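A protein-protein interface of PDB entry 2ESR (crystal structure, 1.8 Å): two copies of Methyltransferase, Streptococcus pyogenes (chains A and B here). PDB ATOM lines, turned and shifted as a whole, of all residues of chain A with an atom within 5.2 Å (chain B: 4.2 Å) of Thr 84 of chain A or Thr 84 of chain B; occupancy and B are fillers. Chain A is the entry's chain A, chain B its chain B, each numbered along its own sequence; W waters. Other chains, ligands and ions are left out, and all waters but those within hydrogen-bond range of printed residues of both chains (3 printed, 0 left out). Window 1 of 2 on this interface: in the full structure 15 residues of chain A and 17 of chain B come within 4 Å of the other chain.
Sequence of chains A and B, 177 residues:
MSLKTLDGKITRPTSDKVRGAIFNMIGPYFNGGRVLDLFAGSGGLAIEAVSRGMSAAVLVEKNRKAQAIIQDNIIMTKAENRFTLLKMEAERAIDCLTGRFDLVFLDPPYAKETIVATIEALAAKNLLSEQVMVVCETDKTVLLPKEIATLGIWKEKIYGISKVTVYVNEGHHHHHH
O of Phe 83 of chain A lies within hydrogen-bond range of NH2 of Arg 34 of chain B, at 3.4 Å.
O of Ala 57 of chain A lies within hydrogen-bond range of N of Thr 84 of chain A (2.9 Å).
The backbone carbonyl oxygen of Thr 84 of chain A is in hydrogen-bond range of the backbone NH of Leu 59 of chain A.
The backbone NH (N) of Leu 86 of chain A sits at hydrogen-bond distance from the backbone carbonyl oxygen (O) of Leu 59 of chain A (2.7 Å).
O of Ala 57 of chain B is in hydrogen-bond range of N of Thr 84 of chain B (2.9 Å).
O of Thr 84 of chain B is in hydrogen-bond range of N of Leu 59 of chain B (2.8 Å).
The backbone carbonyl oxygen (O) of Leu 59 of chain B is in hydrogen-bond range of the backbone NH (N) of Leu 86 of chain B, at 2.7 Å.
OG1 of Thr 84 of chain A touches NH2 of Arg 34 of chain B, at 3.6 Å.
OG1 of Thr 84 of chain B touches OG1 of Thr 84 of chain A, at 3.7 Å.
CD2 of Leu 86 of chain A touches CD1 of Leu 86 of chain B (3.9 Å).
Printed residues of chain B within 4 Å of Phe 83 of chain A: Arg 34 (3.4 Å).
Thr 84 of chain A touches just these residues of chain B: Arg 34 and Thr 84.
Of the printed residues of chain A, Arg 34 of chain B touches Phe 83 (3.4 Å) and Thr 84 (3.6 Å).
Thr 84 of chain B touches just one residue of chain A: Thr 84 (3.7 Å).
Of the printed residues of chain A, Leu 86 of chain B touches Leu 86 (3.9 Å).
The nearest residue of chain B that does not touch Thr 84 of chain A is Val 58 of chain B (4.1 Å).
The nearest residue of chain A that does not touch Thr 84 of chain B is Val 58 of chain A (4.04 Å).
The nearest printed residue of chain A that does not touch Arg 34 of chain B is Leu 85 of chain A (5.3 Å).
Of the 8 printed residues of chain B, 3 touch a printed residue of chain A.
Of the 8 printed residues of chain A, 3 touch a printed residue of chain B.
Hydrophobic or aromatic side chains of chain A that line the printed part of chain B: Leu 86.
Among the printed residues, 4 pairs touch across the chains.
Among the printed residues, no Asp or Glu carboxylate lies within 4 Å of a Lys or Arg side-chain nitrogen of the other chain.
Thr 84 of chain B touches its own counterpart, Thr 84 of chain A.
Leu 86 of chain B touches its own counterpart, Leu 86 of chain A.
Positions printed for both chains: 57, 58, 59, 83, 84, 85 and 86.
Of the 4 pairs that touch across the chains among the printed residues, 2 have their exchanged pair printed and touching as well.
Water W2 bridges the backbone carbonyl oxygen of Phe 83 of chain A (2.7 Å) and the guanidinium group of Arg 34 of chain B (2.8 Å).
Water W3 lies within hydrogen-bond range of the side-chain hydroxyl (OG1) of Thr 84 of chain A (2.8 Å), the side-chain hydroxyl (OG1) of Thr 84 of chain B (3.0 Å) and the backbone carbonyl oxygen (O) of Ala 57 of chain A (3.2 Å).
Water W1 lies within hydrogen-bond range of the backbone NH (N) of Leu 85 of chain A (2.9 Å), the guanidinium group (NH1) of Arg 34 of chain B (3.1 Å) and the backbone carbonyl oxygen (O) of Phe 83 of chain A (3.5 Å).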
ATOM      1  N   ALA A  57      21.214  22.389  26.536  1.00  0.00           N
ATOM      2  CA  ALA A  57      21.142  23.391  25.486  1.00  0.00           C
ATOM      3  C   ALA A  57      20.380  22.896  24.278  1.00  0.00           C
ATOM      4  O   ALA A  57      20.461  21.723  23.911  1.00  0.00           O
ATOM      5  CB  ALA A  57      22.537  23.791  25.060  1.00  0.00           C
ATOM      6  N   VAL A  58      19.621  23.795  23.673  1.00  0.00           N
ATOM      7  CA  VAL A  58      18.900  23.474  22.456  1.00  0.00           C
ATOM      8  C   VAL A  58      19.605  24.341  21.431  1.00  0.00           C
ATOM      9  O   VAL A  58      19.740  25.549  21.629  1.00  0.00           O
ATOM     10  CB  VAL A  58      17.410  23.873  22.510  1.00  0.00           C
ATOM     11  CG1 VAL A  58      16.786  23.723  21.114  1.00  0.00           C
ATOM     12  CG2 VAL A  58      16.668  22.999  23.503  1.00  0.00           C
ATOM     13  N   LEU A  59      20.090  23.724  20.362  1.00  0.00           N
ATOM     14  CA  LEU A  59      20.770  24.464  19.308  1.00  0.00           C
ATOM     15  C   LEU A  59      19.954  24.368  18.028  1.00  0.00           C
ATOM     16  O   LEU A  59      19.451  23.298  17.690  1.00  0.00           O
ATOM     17  CB  LEU A  59      22.172  23.894  19.058  1.00  0.00           C
ATOM     18  CG  LEU A  59      23.235  24.048  20.151  1.00  0.00           C
ATOM     19  CD1 LEU A  59      22.911  23.144  21.337  1.00  0.00           C
ATOM     20  CD2 LEU A  59      24.594  23.697  19.575  1.00  0.00           C
ATOM     21  N   ARG A  82      23.305  16.230  26.841  1.00  0.00           N
ATOM     22  CA  ARG A  82      22.814  17.513  27.333  1.00  0.00           C
ATOM     23  C   ARG A  82      22.447  18.465  26.196  1.00  0.00           C
ATOM     24  O   ARG A  82      21.990  19.583  26.440  1.00  0.00           O
ATOM     25  CB  ARG A  82      23.880  18.172  28.214  1.00  0.00           C
ATOM     26  CG  ARG A  82      24.574  17.213  29.182  1.00  0.00           C
ATOM     27  CD  ARG A  82      25.724  17.897  29.912  1.00  0.00           C
ATOM     28  NE  ARG A  82      25.249  18.842  30.917  1.00  0.00           N
ATOM     29  CZ  ARG A  82      24.732  18.490  32.090  1.00  0.00           C
ATOM     30  NH1 ARG A  82      24.626  17.207  32.417  1.00  0.00           N
ATOM     31  NH2 ARG A  82      24.309  19.422  32.933  1.00  0.00           N
ATOM     32  N   PHE A  83      22.635  18.024  24.957  1.00  0.00           N
ATOM     33  CA  PHE A  83      22.338  18.874  23.811  1.00  0.00           C
ATOM     34  C   PHE A  83      21.273  18.336  22.871  1.00  0.00           C
ATOM     35  O   PHE A  83      21.198  17.137  22.606  1.00  0.00           O
ATOM     36  CB  PHE A  83      23.612  19.131  23.006  1.00  0.00           C
ATOM     37  CG  PHE A  83      24.741  19.673  23.822  1.00  0.00           C
ATOM     38  CD1 PHE A  83      25.575  18.819  24.537  1.00  0.00           C
ATOM     39  CD2 PHE A  83      24.959  21.044  23.902  1.00  0.00           C
ATOM     40  CE1 PHE A  83      26.612  19.321  25.321  1.00  0.00           C
ATOM     41  CE2 PHE A  83      25.991  21.557  24.683  1.00  0.00           C
ATOM     42  CZ  PHE A  83      26.820  20.696  25.393  1.00  0.00           C
ATOM     43  N   THR A  84      20.450  19.249  22.369  1.00  0.00           N
ATOM     44  CA  THR A  84      19.398  18.916  21.426  1.00  0.00           C
ATOM     45  C   THR A  84      19.609  19.832  20.221  1.00  0.00           C
ATOM     46  O   THR A  84      19.517  21.051  20.348  1.00  0.00           O
ATOM     47  CB  THR A  84      18.005  19.178  22.023  1.00  0.00           C
ATOM     48  OG1 THR A  84      17.839  18.397  23.215  1.00  0.00           O
ATOM     49  CG2 THR A  84      16.919  18.807  21.020  1.00  0.00           C
ATOM     50  N   LEU A  85      19.921  19.243  19.067  1.00  0.00           N
ATOM     51  CA  LEU A  85      20.139  20.018  17.852  1.00  0.00           C
ATOM     52  C   LEU A  85      18.936  19.906  16.926  1.00  0.00           C
ATOM     53  O   LEU A  85      18.482  18.809  16.602  1.00  0.00           O
ATOM     54  CB  LEU A  85      21.394  19.541  17.106  1.00  0.00           C
ATOM     55  CG  LEU A  85      21.633  20.217  15.746  1.00  0.00           C
ATOM     56  CD1 LEU A  85      21.950  21.692  15.957  1.00  0.00           C
ATOM     57  CD2 LEU A  85      22.778  19.543  15.005  1.00  0.00           C
ATOM     58  N   LEU A  86      18.422  21.055  16.510  1.00  0.00           N
ATOM     59  CA  LEU A  86      17.280  21.099  15.613  1.00  0.00           C
ATOM     60  C   LEU A  86      17.731  21.689  14.289  1.00  0.00           C
ATOM     61  O   LEU A  86      18.347  22.757  14.252  1.00  0.00           O
ATOM     62  CB  LEU A  86      16.165  21.962  16.203  1.00  0.00           C
ATOM     63  CG  LEU A  86      15.525  21.468  17.504  1.00  0.00           C
ATOM     64  CD1 LEU A  86      14.528  22.498  18.004  1.00  0.00           C
ATOM     65  CD2 LEU A  86      14.839  20.135  17.263  1.00  0.00           C
ATOM     66  N   ARG B  34      19.898   8.764  25.497  1.00  0.00           N
ATOM     67  CA  ARG B  34      18.877   9.729  25.107  1.00  0.00           C
ATOM     68  C   ARG B  34      17.573   9.049  24.719  1.00  0.00           C
ATOM     69  O   ARG B  34      17.566   8.053  23.995  1.00  0.00           O
ATOM     70  CB  ARG B  34      19.352  10.570  23.928  1.00  0.00           C
ATOM     71  CG  ARG B  34      20.612  11.366  24.183  1.00  0.00           C
ATOM     72  CD  ARG B  34      20.826  12.345  23.041  1.00  0.00           C
ATOM     73  NE  ARG B  34      19.817  13.401  23.052  1.00  0.00           N
ATOM     74  CZ  ARG B  34      19.500  14.147  21.997  1.00  0.00           C
ATOM     75  NH1 ARG B  34      20.109  13.950  20.835  1.00  0.00           N
ATOM     76  NH2 ARG B  34      18.585  15.100  22.109  1.00  0.00           N
ATOM     77  N   ALA B  57      15.752  13.320  27.766  1.00  0.00           N
ATOM     78  CA  ALA B  57      14.634  12.936  26.923  1.00  0.00           C
ATOM     79  C   ALA B  57      14.055  14.102  26.147  1.00  0.00           C
ATOM     80  O   ALA B  57      13.937  15.216  26.662  1.00  0.00           O
ATOM     81  CB  ALA B  57      13.538  12.296  27.767  1.00  0.00           C
ATOM     82  N   VAL B  58      13.706  13.829  24.895  1.00  0.00           N
ATOM     83  CA  VAL B  58      13.078  14.813  24.028  1.00  0.00           C
ATOM     84  C   VAL B  58      11.645  14.323  23.905  1.00  0.00           C
ATOM     85  O   VAL B  58      11.400  13.187  23.487  1.00  0.00           O
ATOM     86  CB  VAL B  58      13.721  14.858  22.627  1.00  0.00           C
ATOM     87  CG1 VAL B  58      12.898  15.750  21.707  1.00  0.00           C
ATOM     88  CG2 VAL B  58      15.150  15.381  22.732  1.00  0.00           C
ATOM     89  N   LEU B  59      10.711  15.177  24.300  1.00  0.00           N
ATOM     90  CA  LEU B  59       9.297  14.853  24.262  1.00  0.00           C
ATOM     91  C   LEU B  59       8.625  15.644  23.154  1.00  0.00           C
ATOM     92  O   LEU B  59       8.842  16.846  23.022  1.00  0.00           O
ATOM     93  CB  LEU B  59       8.634  15.193  25.608  1.00  0.00           C
ATOM     94  CG  LEU B  59       8.922  14.274  26.806  1.00  0.00           C
ATOM     95  CD1 LEU B  59      10.387  14.334  27.180  1.00  0.00           C
ATOM     96  CD2 LEU B  59       8.062  14.700  27.986  1.00  0.00           C
ATOM     97  N   PHE B  83      14.794  17.258  30.444  1.00  0.00           N
ATOM     98  CA  PHE B  83      13.672  17.080  29.536  1.00  0.00           C
ATOM     99  C   PHE B  83      13.481  18.255  28.590  1.00  0.00           C
ATOM    100  O   PHE B  83      13.492  19.415  29.006  1.00  0.00           O
ATOM    101  CB  PHE B  83      12.400  16.860  30.352  1.00  0.00           C
ATOM    102  CG  PHE B  83      12.485  15.700  31.292  1.00  0.00           C
ATOM    103  CD1 PHE B  83      12.306  14.400  30.829  1.00  0.00           C
ATOM    104  CD2 PHE B  83      12.762  15.901  32.641  1.00  0.00           C
ATOM    105  CE1 PHE B  83      12.402  13.321  31.692  1.00  0.00           C
ATOM    106  CE2 PHE B  83      12.861  14.827  33.515  1.00  0.00           C
ATOM    107  CZ  PHE B  83      12.679  13.533  33.040  1.00  0.00           C
ATOM    108  N   THR B  84      13.309  17.946  27.311  1.00  0.00           N
ATOM    109  CA  THR B  84      13.106  18.965  26.295  1.00  0.00           C
ATOM    110  C   THR B  84      11.781  18.710  25.586  1.00  0.00           C
ATOM    111  O   THR B  84      11.628  17.720  24.870  1.00  0.00           O
ATOM    112  CB  THR B  84      14.247  18.943  25.265  1.00  0.00           C
ATOM    113  OG1 THR B  84      15.491  19.183  25.935  1.00  0.00           O
ATOM    114  CG2 THR B  84      14.033  20.014  24.200  1.00  0.00           C
ATOM    115  N   LEU B  85      10.823  19.606  25.794  1.00  0.00           N
ATOM    116  CA  LEU B  85       9.510  19.467  25.177  1.00  0.00           C
ATOM    117  C   LEU B  85       9.380  20.249  23.879  1.00  0.00           C
ATOM    118  O   LEU B  85       9.654  21.453  23.831  1.00  0.00           O
ATOM    119  CB  LEU B  85       8.417  19.919  26.152  1.00  0.00           C
ATOM    120  CG  LEU B  85       6.975  19.931  25.627  1.00  0.00           C
ATOM    121  CD1 LEU B  85       6.544  18.522  25.223  1.00  0.00           C
ATOM    122  CD2 LEU B  85       6.057  20.473  26.701  1.00  0.00           C
ATOM    123  N   LEU B  86       8.965  19.553  22.825  1.00  0.00           N
ATOM    124  CA  LEU B  86       8.775  20.173  21.522  1.00  0.00           C
ATOM    125  C   LEU B  86       7.309  20.054  21.127  1.00  0.00           C
ATOM    126  O   LEU B  86       6.741  18.961  21.115  1.00  0.00           O
ATOM    127  CB  LEU B  86       9.647  19.499  20.463  1.00  0.00           C
ATOM    128  CG  LEU B  86      11.160  19.615  20.666  1.00  0.00           C
ATOM    129  CD1 LEU B  86      11.868  18.908  19.520  1.00  0.00           C
ATOM    130  CD2 LEU B  86      11.572  21.081  20.739  1.00  0.00           C
HETATM  131  O   HOH W   1      20.840  16.538  19.214  1.00  0.00           O
HETATM  132  O   HOH W   2      22.561  14.940  21.866  1.00  0.00           O
HETATM  133  O   HOH W   3      18.407  19.910  25.511  1.00  0.00           O
